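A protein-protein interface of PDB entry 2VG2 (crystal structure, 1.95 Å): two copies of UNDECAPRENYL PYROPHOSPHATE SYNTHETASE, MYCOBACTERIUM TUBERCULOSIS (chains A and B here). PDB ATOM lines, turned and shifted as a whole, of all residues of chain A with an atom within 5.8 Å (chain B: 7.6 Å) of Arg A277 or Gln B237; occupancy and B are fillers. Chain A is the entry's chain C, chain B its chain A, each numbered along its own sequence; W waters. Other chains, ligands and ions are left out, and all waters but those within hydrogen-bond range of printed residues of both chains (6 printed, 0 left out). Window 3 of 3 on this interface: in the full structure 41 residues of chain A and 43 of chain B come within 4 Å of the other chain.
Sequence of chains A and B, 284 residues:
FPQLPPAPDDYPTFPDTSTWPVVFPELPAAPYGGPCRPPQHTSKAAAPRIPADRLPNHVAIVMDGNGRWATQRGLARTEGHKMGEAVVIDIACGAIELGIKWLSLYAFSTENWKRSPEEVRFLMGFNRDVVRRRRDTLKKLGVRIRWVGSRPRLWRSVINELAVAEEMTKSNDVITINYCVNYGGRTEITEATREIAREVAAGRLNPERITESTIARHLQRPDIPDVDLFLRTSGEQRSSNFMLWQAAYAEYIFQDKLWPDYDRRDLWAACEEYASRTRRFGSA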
ATOM      1  N   ARG A  54       2.354  -7.442  -8.760  1.00  0.00           N
ATOM      2  CA  ARG A  54       1.075  -6.721  -8.871  1.00  0.00           C
ATOM      3  C   ARG A  54      -0.038  -7.573  -9.486  1.00  0.00           C
ATOM      4  O   ARG A  54      -1.179  -7.121  -9.619  1.00  0.00           O
ATOM      5  CB  ARG A  54       1.255  -5.423  -9.671  1.00  0.00           C
ATOM      6  CG  ARG A  54       1.933  -4.287  -8.889  1.00  0.00           C
ATOM      7  CD  ARG A  54       1.230  -4.086  -7.548  1.00  0.00           C
ATOM      8  NE  ARG A  54       1.363  -2.739  -7.008  1.00  0.00           N
ATOM      9  CZ  ARG A  54       0.669  -2.273  -5.969  1.00  0.00           C
ATOM     10  NH1 ARG A  54      -0.223  -3.039  -5.354  1.00  0.00           N
ATOM     11  NH2 ARG A  54       0.862  -1.030  -5.542  1.00  0.00           N
ATOM     12  N   ALA A 250     -10.272 -10.338  -0.348  1.00  0.00           N
ATOM     13  CA  ALA A 250     -10.200 -10.117  -1.793  1.00  0.00           C
ATOM     14  C   ALA A 250     -10.564  -8.687  -2.204  1.00  0.00           C
ATOM     15  O   ALA A 250     -11.387  -8.038  -1.556  1.00  0.00           O
ATOM     16  CB  ALA A 250     -11.110 -11.094  -2.512  1.00  0.00           C
ATOM     17  N   GLU A 251      -9.950  -8.213  -3.287  1.00  0.00           N
ATOM     18  CA  GLU A 251     -10.402  -7.004  -3.978  1.00  0.00           C
ATOM     19  C   GLU A 251     -11.566  -7.362  -4.887  1.00  0.00           C
ATOM     20  O   GLU A 251     -11.490  -8.368  -5.612  1.00  0.00           O
ATOM     21  CB  GLU A 251      -9.271  -6.414  -4.826  1.00  0.00           C
ATOM     22  CG  GLU A 251      -8.065  -5.942  -4.028  1.00  0.00           C
ATOM     23  CD  GLU A 251      -8.351  -4.719  -3.175  1.00  0.00           C
ATOM     24  OE1 GLU A 251      -9.086  -3.818  -3.632  1.00  0.00           O
ATOM     25  OE2 GLU A 251      -7.821  -4.652  -2.047  1.00  0.00           O
ATOM     26  N   TYR A 252     -12.620  -6.536  -4.857  1.00  0.00           N
ATOM     27  CA  TYR A 252     -13.802  -6.714  -5.720  1.00  0.00           C
ATOM     28  C   TYR A 252     -13.742  -5.809  -6.934  1.00  0.00           C
ATOM     29  O   TYR A 252     -13.465  -4.617  -6.810  1.00  0.00           O
ATOM     30  CB  TYR A 252     -15.103  -6.389  -4.969  1.00  0.00           C
ATOM     31  CG  TYR A 252     -15.456  -7.391  -3.905  1.00  0.00           C
ATOM     32  CD1 TYR A 252     -15.820  -8.681  -4.247  1.00  0.00           C
ATOM     33  CD2 TYR A 252     -15.459  -7.041  -2.560  1.00  0.00           C
ATOM     34  CE1 TYR A 252     -16.151  -9.610  -3.281  1.00  0.00           C
ATOM     35  CE2 TYR A 252     -15.775  -7.973  -1.578  1.00  0.00           C
ATOM     36  CZ  TYR A 252     -16.119  -9.247  -1.946  1.00  0.00           C
ATOM     37  OH  TYR A 252     -16.459 -10.188  -1.016  1.00  0.00           O
ATOM     38  N   ILE A 253     -14.025  -6.386  -8.094  1.00  0.00           N
ATOM     39  CA  ILE A 253     -14.274  -5.624  -9.307  1.00  0.00           C
ATOM     40  C   ILE A 253     -15.588  -6.116  -9.887  1.00  0.00           C
ATOM     41  O   ILE A 253     -15.767  -7.316 -10.151  1.00  0.00           O
ATOM     42  CB  ILE A 253     -13.126  -5.765 -10.309  1.00  0.00           C
ATOM     43  CG1 ILE A 253     -11.886  -5.051  -9.771  1.00  0.00           C
ATOM     44  CG2 ILE A 253     -13.495  -5.162 -11.664  1.00  0.00           C
ATOM     45  CD1 ILE A 253     -10.710  -5.060 -10.719  1.00  0.00           C
ATOM     46  N   PHE A 254     -16.525  -5.188 -10.037  1.00  0.00           N
ATOM     47  CA  PHE A 254     -17.841  -5.499 -10.583  1.00  0.00           C
ATOM     48  C   PHE A 254     -17.975  -4.872 -11.959  1.00  0.00           C
ATOM     49  O   PHE A 254     -18.037  -3.656 -12.090  1.00  0.00           O
ATOM     50  CB  PHE A 254     -18.922  -4.986  -9.637  1.00  0.00           C
ATOM     51  CG  PHE A 254     -18.922  -5.676  -8.306  1.00  0.00           C
ATOM     52  CD1 PHE A 254     -19.210  -7.025  -8.223  1.00  0.00           C
ATOM     53  CD2 PHE A 254     -18.616  -4.993  -7.140  1.00  0.00           C
ATOM     54  CE1 PHE A 254     -19.192  -7.685  -6.996  1.00  0.00           C
ATOM     55  CE2 PHE A 254     -18.613  -5.651  -5.913  1.00  0.00           C
ATOM     56  CZ  PHE A 254     -18.907  -6.984  -5.848  1.00  0.00           C
ATOM     57  N   GLU A 273      -6.763  -3.143 -13.319  1.00  0.00           N
ATOM     58  CA  GLU A 273      -7.373  -2.345 -12.263  1.00  0.00           C
ATOM     59  C   GLU A 273      -6.850  -2.840 -10.916  1.00  0.00           C
ATOM     60  O   GLU A 273      -6.387  -2.052 -10.103  1.00  0.00           O
ATOM     61  CB  GLU A 273      -8.903  -2.423 -12.329  1.00  0.00           C
ATOM     62  CG  GLU A 273      -9.607  -1.128 -11.950  1.00  0.00           C
ATOM     63  CD  GLU A 273     -11.090  -1.333 -11.649  1.00  0.00           C
ATOM     64  OE1 GLU A 273     -11.842  -1.760 -12.565  1.00  0.00           O
ATOM     65  OE2 GLU A 273     -11.506  -1.056 -10.500  1.00  0.00           O
ATOM     66  N   TYR A 274      -6.901  -4.154 -10.703  1.00  0.00           N
ATOM     67  CA  TYR A 274      -6.311  -4.772  -9.515  1.00  0.00           C
ATOM     68  C   TYR A 274      -4.871  -4.305  -9.269  1.00  0.00           C
ATOM     69  O   TYR A 274      -4.519  -3.943  -8.150  1.00  0.00           O
ATOM     70  CB  TYR A 274      -6.353  -6.303  -9.630  1.00  0.00           C
ATOM     71  CG  TYR A 274      -5.621  -7.019  -8.516  1.00  0.00           C
ATOM     72  CD1 TYR A 274      -6.258  -7.323  -7.321  1.00  0.00           C
ATOM     73  CD2 TYR A 274      -4.287  -7.379  -8.660  1.00  0.00           C
ATOM     74  CE1 TYR A 274      -5.581  -7.955  -6.296  1.00  0.00           C
ATOM     75  CE2 TYR A 274      -3.610  -8.014  -7.653  1.00  0.00           C
ATOM     76  CZ  TYR A 274      -4.260  -8.302  -6.476  1.00  0.00           C
ATOM     77  OH  TYR A 274      -3.571  -8.933  -5.487  1.00  0.00           O
ATOM     78  N   ALA A 275      -4.064  -4.292 -10.330  1.00  0.00           N
ATOM     79  CA  ALA A 275      -2.601  -4.088 -10.236  1.00  0.00           C
ATOM     80  C   ALA A 275      -2.139  -2.771  -9.596  1.00  0.00           C
ATOM     81  O   ALA A 275      -0.982  -2.646  -9.186  1.00  0.00           O
ATOM     82  CB  ALA A 275      -1.976  -4.227 -11.617  1.00  0.00           C
ATOM     83  N   SER A 276      -3.021  -1.783  -9.521  1.00  0.00           N
ATOM     84  CA  SER A 276      -2.665  -0.507  -8.915  1.00  0.00           C
ATOM     85  C   SER A 276      -3.576  -0.123  -7.758  1.00  0.00           C
ATOM     86  O   SER A 276      -3.652   1.050  -7.389  1.00  0.00           O
ATOM     87  CB  SER A 276      -2.703   0.579  -9.977  1.00  0.00           C
ATOM     88  OG  SER A 276      -4.020   0.692 -10.492  1.00  0.00           O
ATOM     89  N   ARG A 277      -4.265  -1.104  -7.189  1.00  0.00           N
ATOM     90  CA  ARG A 277      -4.935  -0.924  -5.914  1.00  0.00           C
ATOM     91  C   ARG A 277      -3.955  -1.256  -4.807  1.00  0.00           C
ATOM     92  O   ARG A 277      -3.117  -2.153  -4.962  1.00  0.00           O
ATOM     93  CB  ARG A 277      -6.144  -1.843  -5.801  1.00  0.00           C
ATOM     94  CG  ARG A 277      -7.269  -1.477  -6.748  1.00  0.00           C
ATOM     95  CD  ARG A 277      -8.570  -1.883  -6.146  1.00  0.00           C
ATOM     96  NE  ARG A 277      -9.684  -1.817  -7.081  1.00  0.00           N
ATOM     97  CZ  ARG A 277     -10.819  -2.501  -6.940  1.00  0.00           C
ATOM     98  NH1 ARG A 277     -10.993  -3.319  -5.906  1.00  0.00           N
ATOM     99  NH2 ARG A 277     -11.777  -2.372  -7.846  1.00  0.00           N
ATOM    100  N   THR A 278      -4.063  -0.540  -3.693  1.00  0.00           N
ATOM    101  CA  THR A 278      -3.225  -0.812  -2.534  1.00  0.00           C
ATOM    102  C   THR A 278      -3.970  -1.724  -1.577  1.00  0.00           C
ATOM    103  O   THR A 278      -5.051  -1.375  -1.105  1.00  0.00           O
ATOM    104  CB  THR A 278      -2.850   0.469  -1.803  1.00  0.00           C
ATOM    105  OG1 THR A 278      -2.038   1.277  -2.664  1.00  0.00           O
ATOM    106  CG2 THR A 278      -2.078   0.142  -0.530  1.00  0.00           C
ATOM    107  N   ARG A 279      -3.390  -2.888  -1.302  1.00  0.00           N
ATOM    108  CA  ARG A 279      -3.933  -3.817  -0.316  1.00  0.00           C
ATOM    109  C   ARG A 279      -3.183  -3.621   0.996  1.00  0.00           C
ATOM    110  O   ARG A 279      -1.973  -3.333   0.992  1.00  0.00           O
ATOM    111  CB  ARG A 279      -3.808  -5.256  -0.811  1.00  0.00           C
ATOM    112  CG  ARG A 279      -4.346  -5.456  -2.219  1.00  0.00           C
ATOM    113  CD  ARG A 279      -4.252  -6.915  -2.664  1.00  0.00           C
ATOM    114  NE  ARG A 279      -5.269  -7.750  -2.029  1.00  0.00           N
ATOM    115  CZ  ARG A 279      -5.256  -9.081  -2.017  1.00  0.00           C
ATOM    116  NH1 ARG A 279      -4.279  -9.764  -2.602  1.00  0.00           N
ATOM    117  NH2 ARG A 279      -6.232  -9.739  -1.405  1.00  0.00           N
ATOM    118  N   ASP B  64     -13.917   3.731   6.647  1.00  0.00           N
ATOM    119  CA  ASP B  64     -12.559   3.818   6.144  1.00  0.00           C
ATOM    120  C   ASP B  64     -12.208   5.244   5.749  1.00  0.00           C
ATOM    121  O   ASP B  64     -13.087   5.996   5.331  1.00  0.00           O
ATOM    122  CB  ASP B  64     -12.493   2.920   4.912  1.00  0.00           C
ATOM    123  CG  ASP B  64     -11.162   2.268   4.722  1.00  0.00           C
ATOM    124  OD1 ASP B  64     -10.172   2.647   5.403  1.00  0.00           O
ATOM    125  OD2 ASP B  64     -11.100   1.392   3.840  1.00  0.00           O
ATOM    126  N   ARG B 232     -18.922   0.763   2.279  1.00  0.00           N
ATOM    127  CA  ARG B 232     -17.570   1.115   2.648  1.00  0.00           C
ATOM    128  C   ARG B 232     -17.215   2.440   2.037  1.00  0.00           C
ATOM    129  O   ARG B 232     -17.543   2.695   0.888  1.00  0.00           O
ATOM    130  CB  ARG B 232     -16.594   0.050   2.195  1.00  0.00           C
ATOM    131  CG  ARG B 232     -15.151   0.380   2.554  1.00  0.00           C
ATOM    132  CD  ARG B 232     -14.352  -0.888   2.560  1.00  0.00           C
ATOM    133  NE  ARG B 232     -13.001  -0.676   3.042  1.00  0.00           N
ATOM    134  CZ  ARG B 232     -12.236  -1.653   3.506  1.00  0.00           C
ATOM    135  NH1 ARG B 232     -12.698  -2.896   3.514  1.00  0.00           N
ATOM    136  NH2 ARG B 232     -11.012  -1.404   3.947  1.00  0.00           N
ATOM    137  N   THR B 233     -16.543   3.279   2.820  1.00  0.00           N
ATOM    138  CA  THR B 233     -16.126   4.609   2.375  1.00  0.00           C
ATOM    139  C   THR B 233     -14.666   4.594   1.897  1.00  0.00           C
ATOM    140  O   THR B 233     -13.998   3.564   1.958  1.00  0.00           O
ATOM    141  CB  THR B 233     -16.334   5.633   3.511  1.00  0.00           C
ATOM    142  OG1 THR B 233     -15.721   5.159   4.715  1.00  0.00           O
ATOM    143  CG2 THR B 233     -17.809   5.817   3.773  1.00  0.00           C
ATOM    144  N   SER B 234     -14.203   5.734   1.401  1.00  0.00           N
ATOM    145  CA  SER B 234     -12.814   5.962   0.963  1.00  0.00           C
ATOM    146  C   SER B 234     -12.424   5.371  -0.408  1.00  0.00           C
ATOM    147  O   SER B 234     -11.269   5.496  -0.827  1.00  0.00           O
ATOM    148  CB  SER B 234     -11.813   5.530   2.036  1.00  0.00           C
ATOM    149  OG  SER B 234     -11.503   4.153   1.913  1.00  0.00           O
ATOM    150  N   GLY B 235     -13.376   4.765  -1.118  1.00  0.00           N
ATOM    151  CA  GLY B 235     -13.118   4.246  -2.468  1.00  0.00           C
ATOM    152  C   GLY B 235     -12.542   2.838  -2.501  1.00  0.00           C
ATOM    153  O   GLY B 235     -12.233   2.318  -3.570  1.00  0.00           O
ATOM    154  N   GLU B 236     -12.390   2.215  -1.336  1.00  0.00           N
ATOM    155  CA  GLU B 236     -11.876   0.853  -1.247  1.00  0.00           C
ATOM    156  C   GLU B 236     -13.009  -0.107  -1.552  1.00  0.00           C
ATOM    157  O   GLU B 236     -14.130   0.094  -1.077  1.00  0.00           O
ATOM    158  CB  GLU B 236     -11.320   0.566   0.158  1.00  0.00           C
ATOM    159  CG  GLU B 236     -10.158   1.490   0.581  1.00  0.00           C
ATOM    160  CD  GLU B 236      -8.906   1.342  -0.263  1.00  0.00           C
ATOM    161  OE1 GLU B 236      -7.998   2.198  -0.129  1.00  0.00           O
ATOM    162  OE2 GLU B 236      -8.804   0.377  -1.059  1.00  0.00           O
ATOM    163  N   GLN B 237     -12.717  -1.127  -2.350  1.00  0.00           N
ATOM    164  CA  GLN B 237     -13.709  -2.130  -2.717  1.00  0.00           C
ATOM    165  C   GLN B 237     -13.261  -3.508  -2.243  1.00  0.00           C
ATOM    166  O   GLN B 237     -12.688  -4.292  -2.992  1.00  0.00           O
ATOM    167  CB  GLN B 237     -13.969  -2.123  -4.225  1.00  0.00           C
ATOM    168  CG  GLN B 237     -14.425  -0.772  -4.738  1.00  0.00           C
ATOM    169  CD  GLN B 237     -14.952  -0.778  -6.157  1.00  0.00           C
ATOM    170  OE1 GLN B 237     -15.430   0.245  -6.622  1.00  0.00           O
ATOM    171  NE2 GLN B 237     -14.871  -1.918  -6.853  1.00  0.00           N
ATOM    172  N   ARG B 238     -13.519  -3.754  -0.971  1.00  0.00           N
ATOM    173  CA  ARG B 238     -13.245  -5.023  -0.325  1.00  0.00           C
ATOM    174  C   ARG B 238     -14.087  -5.067   0.936  1.00  0.00           C
ATOM    175  O   ARG B 238     -14.506  -4.017   1.453  1.00  0.00           O
ATOM    176  CB  ARG B 238     -11.750  -5.169  -0.022  1.00  0.00           C
ATOM    177  CG  ARG B 238     -11.081  -3.912   0.471  1.00  0.00           C
ATOM    178  CD  ARG B 238      -9.627  -4.179   0.845  1.00  0.00           C
ATOM    179  NE  ARG B 238      -8.959  -2.995   1.393  1.00  0.00           N
ATOM    180  CZ  ARG B 238      -8.115  -2.208   0.729  1.00  0.00           C
ATOM    181  NH1 ARG B 238      -7.819  -2.427  -0.547  1.00  0.00           N
ATOM    182  NH2 ARG B 238      -7.547  -1.184   1.349  1.00  0.00           N
ATOM    183  N   SER B 239     -14.367  -6.272   1.419  1.00  0.00           N
ATOM    184  CA  SER B 239     -15.161  -6.451   2.632  1.00  0.00           C
ATOM    185  C   SER B 239     -14.248  -6.614   3.863  1.00  0.00           C
ATOM    186  O   SER B 239     -14.694  -6.448   4.992  1.00  0.00           O
ATOM    187  CB  SER B 239     -16.075  -7.670   2.504  1.00  0.00           C
ATOM    188  OG  SER B 239     -15.330  -8.863   2.399  1.00  0.00           O
ATOM    189  N   SER B 240     -12.983  -6.960   3.634  1.00  0.00           N
ATOM    190  CA  SER B 240     -11.987  -7.014   4.705  1.00  0.00           C
ATOM    191  C   SER B 240     -12.441  -7.829   5.926  1.00  0.00           C
ATOM    192  O   SER B 240     -12.272  -7.398   7.063  1.00  0.00           O
ATOM    193  CB  SER B 240     -11.585  -5.604   5.132  1.00  0.00           C
ATOM    194  OG  SER B 240     -10.824  -4.941   4.129  1.00  0.00           O
ATOM    195  N   TYR B 252     -23.297  -4.744  -2.070  1.00  0.00           N
ATOM    196  CA  TYR B 252     -22.243  -3.768  -1.742  1.00  0.00           C
ATOM    197  C   TYR B 252     -22.472  -2.432  -2.444  1.00  0.00           C
ATOM    198  O   TYR B 252     -22.760  -2.394  -3.649  1.00  0.00           O
ATOM    199  CB  TYR B 252     -20.875  -4.320  -2.168  1.00  0.00           C
ATOM    200  CG  TYR B 252     -20.405  -5.468  -1.328  1.00  0.00           C
ATOM    201  CD1 TYR B 252     -19.671  -5.243  -0.185  1.00  0.00           C
ATOM    202  CD2 TYR B 252     -20.683  -6.778  -1.672  1.00  0.00           C
ATOM    203  CE1 TYR B 252     -19.231  -6.275   0.598  1.00  0.00           C
ATOM    204  CE2 TYR B 252     -20.231  -7.845  -0.868  1.00  0.00           C
ATOM    205  CZ  TYR B 252     -19.512  -7.574   0.261  1.00  0.00           C
ATOM    206  OH  TYR B 252     -19.038  -8.581   1.088  1.00  0.00           O
ATOM    207  N   ILE B 253     -22.353  -1.346  -1.686  1.00  0.00           N
ATOM    208  CA  ILE B 253     -22.223  -0.009  -2.263  1.00  0.00           C
ATOM    209  C   ILE B 253     -20.957   0.643  -1.708  1.00  0.00           C
ATOM    210  O   ILE B 253     -20.747   0.709  -0.501  1.00  0.00           O
ATOM    211  CB  ILE B 253     -23.474   0.886  -2.026  1.00  0.00           C
ATOM    212  CG1 ILE B 253     -24.708   0.248  -2.698  1.00  0.00           C
ATOM    213  CG2 ILE B 253     -23.200   2.327  -2.550  1.00  0.00           C
ATOM    214  CD1 ILE B 253     -26.056   1.003  -2.446  1.00  0.00           C
ATOM    215  N   PHE B 254     -20.099   1.086  -2.617  1.00  0.00           N
ATOM    216  CA  PHE B 254     -18.817   1.655  -2.265  1.00  0.00           C
ATOM    217  C   PHE B 254     -18.890   3.146  -2.511  1.00  0.00           C
ATOM    218  O   PHE B 254     -19.168   3.574  -3.630  1.00  0.00           O
ATOM    219  CB  PHE B 254     -17.735   1.025  -3.126  1.00  0.00           C
ATOM    220  CG  PHE B 254     -17.615  -0.458  -2.955  1.00  0.00           C
ATOM    221  CD1 PHE B 254     -17.324  -1.004  -1.710  1.00  0.00           C
ATOM    222  CD2 PHE B 254     -17.756  -1.309  -4.039  1.00  0.00           C
ATOM    223  CE1 PHE B 254     -17.204  -2.368  -1.544  1.00  0.00           C
ATOM    224  CE2 PHE B 254     -17.622  -2.683  -3.872  1.00  0.00           C
ATOM    225  CZ  PHE B 254     -17.346  -3.208  -2.632  1.00  0.00           C
ATOM    226  N   GLN B 255     -18.666   3.940  -1.468  1.00  0.00           N
ATOM    227  CA  GLN B 255     -18.740   5.391  -1.579  1.00  0.00           C
ATOM    228  C   GLN B 255     -17.336   5.955  -1.461  1.00  0.00           C
ATOM    229  O   GLN B 255     -16.537   5.480  -0.656  1.00  0.00           O
ATOM    230  CB  GLN B 255     -19.687   5.957  -0.521  1.00  0.00           C
ATOM    231  CG  GLN B 255     -21.163   5.604  -0.812  1.00  0.00           C
ATOM    232  CD  GLN B 255     -22.104   5.838   0.373  1.00  0.00           C
ATOM    233  OE1 GLN B 255     -22.002   5.180   1.406  1.00  0.00           O
ATOM    234  NE2 GLN B 255     -23.041   6.762   0.203  1.00  0.00           N
ATOM    235  N   ASP B 256     -17.035   6.943  -2.290  1.00  0.00           N
ATOM    236  CA  ASP B 256     -15.665   7.440  -2.430  1.00  0.00           C
ATOM    237  C   ASP B 256     -15.199   8.296  -1.267  1.00  0.00           C
ATOM    238  O   ASP B 256     -14.005   8.346  -0.974  1.00  0.00           O
ATOM    239  CB  ASP B 256     -15.509   8.263  -3.718  1.00  0.00           C
ATOM    240  CG  ASP B 256     -15.509   7.415  -4.958  1.00  0.00           C
ATOM    241  OD1 ASP B 256     -15.189   6.213  -4.872  1.00  0.00           O
ATOM    242  OD2 ASP B 256     -15.813   7.971  -6.037  1.00  0.00           O
HETATM  243  O   HOH W   1     -12.510  -8.337   0.776  1.00  0.00           O
HETATM  244  O   HOH W   2     -16.064  -2.386  -9.280  1.00  0.00           O
HETATM  245  O   HOH W   3      -6.621   0.617  -3.392  1.00  0.00           O
HETATM  246  O   HOH W   4      -9.784  -1.359  -3.067  1.00  0.00           O
HETATM  247  O   HOH W   5     -10.711   0.474  -4.780  1.00  0.00           O
HETATM  248  O   HOH W   6     -15.262 -10.872   1.042  1.00  0.00           O
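The backbone NH (N) of Tyr A252 sits at hydrogen-bond distance from the backbone carbonyl oxygen (O) of Gln B237. NE2 of Gln B237 lies close to NH2 of Arg A277. The guanidinium group (NH1) of Arg B238 is in salt-bridge range of the side-chain carboxylate (OE2) of Glu A251 (2.7 Å). The backbone carbonyl oxygen (O) of Thr A278 is in hydrogen-bond range of the guanidinium group (NH1) of Arg B238 (3.0 Å).
NH1 of Arg B232 sits at hydrogen-bond distance from O of Arg B238, at 3.0 Å. OE2 of Glu B236 lies within salt-bridge range of NH1 of Arg B238 (3.0 Å). The guanidinium group (NH1) of Arg A54 sits at hydrogen-bond distance from the backbone carbonyl oxygen (O) of Arg A277. OE1 of Glu A251 lies within salt-bridge range of NH1 of Arg A277 (3.0 Å). The guanidinium group (NH1) of Arg A277 is in hydrogen-bond range of the backbone carbonyl oxygen (O) of Tyr A252 (2.9 Å). The guanidinium group (NH2) of Arg A277 lies within salt-bridge range of the side-chain carboxylate (OE2) of Glu A273, at 3.0 Å.
Among the printed residues, pairs that only touch across the chains: Ala A250 with Arg B238, Glu A251 with Gln B237, Tyr A252 with Arg B238, Tyr A252 with Ser B239, Tyr A252 with Tyr B252 and Phe A254 with Phe B254.
Printed residues of chain B within 4 Å of Ala A250: Arg B238. Printed residues of chain B within 4 Å of Glu A251: Gln B237 (3.7 Å) and Arg B238 (2.7 Å). Glu A273 touches none of the printed residues of chain B. Arg A277 touches one residue of chain B. Arg B232 touches none of the printed residues of chain A. The nearest residue of chain A that does not touch Gln B237 is Ala A250 (4.2 Å). The nearest printed residue of chain B that does not touch Tyr A252 is Phe B254 (4.3 Å).
Of the 13 printed residues of chain A, 6 touch a printed residue of chain B. Hydrophobic or aromatic side chains of chain A that line the printed part of chain B: Tyr A252 and Phe A254. Of the 15 printed residues of chain B, 5 touch a printed residue of chain A.
Tyr B252 touches its own counterpart, Tyr A252. Phe A254 touches its own counterpart, Phe B254. Of the 10 pairs that touch across the chains among the printed residues, 2 have their exchanged pair printed and touching as well.
Water W6 bridges the side-chain hydroxyl (OG) of Ser B239 and the side-chain hydroxyl (OH) of Tyr A252. Water W1 lies within hydrogen-bond range of O of Ala A250 (2.6 Å), N of Ser B239 (2.9 Å) and N of Ser B240 (3.2 Å). Water W4 lies within hydrogen-bond range of the side-chain carboxylate (OE1) of Glu A251 (2.6 Å), the side-chain carboxylate (OE2) of Glu B236 (2.8 Å), the backbone NH (N) of Gln B237 (3.0 Å) and the guanidinium group (NH1) of Arg B238 (3.4 Å). Water W5 bridges O of Gly B235 and NE of Arg A277. Water W2 bridges NE2 of Gln B237 (2.7 Å) and N of Phe A254 (2.9 Å). Water W3 bridges the backbone NH (N) of Thr A278 (2.8 Å) and the side-chain carboxylate (OE2) of Glu B236 (3.2 Å).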
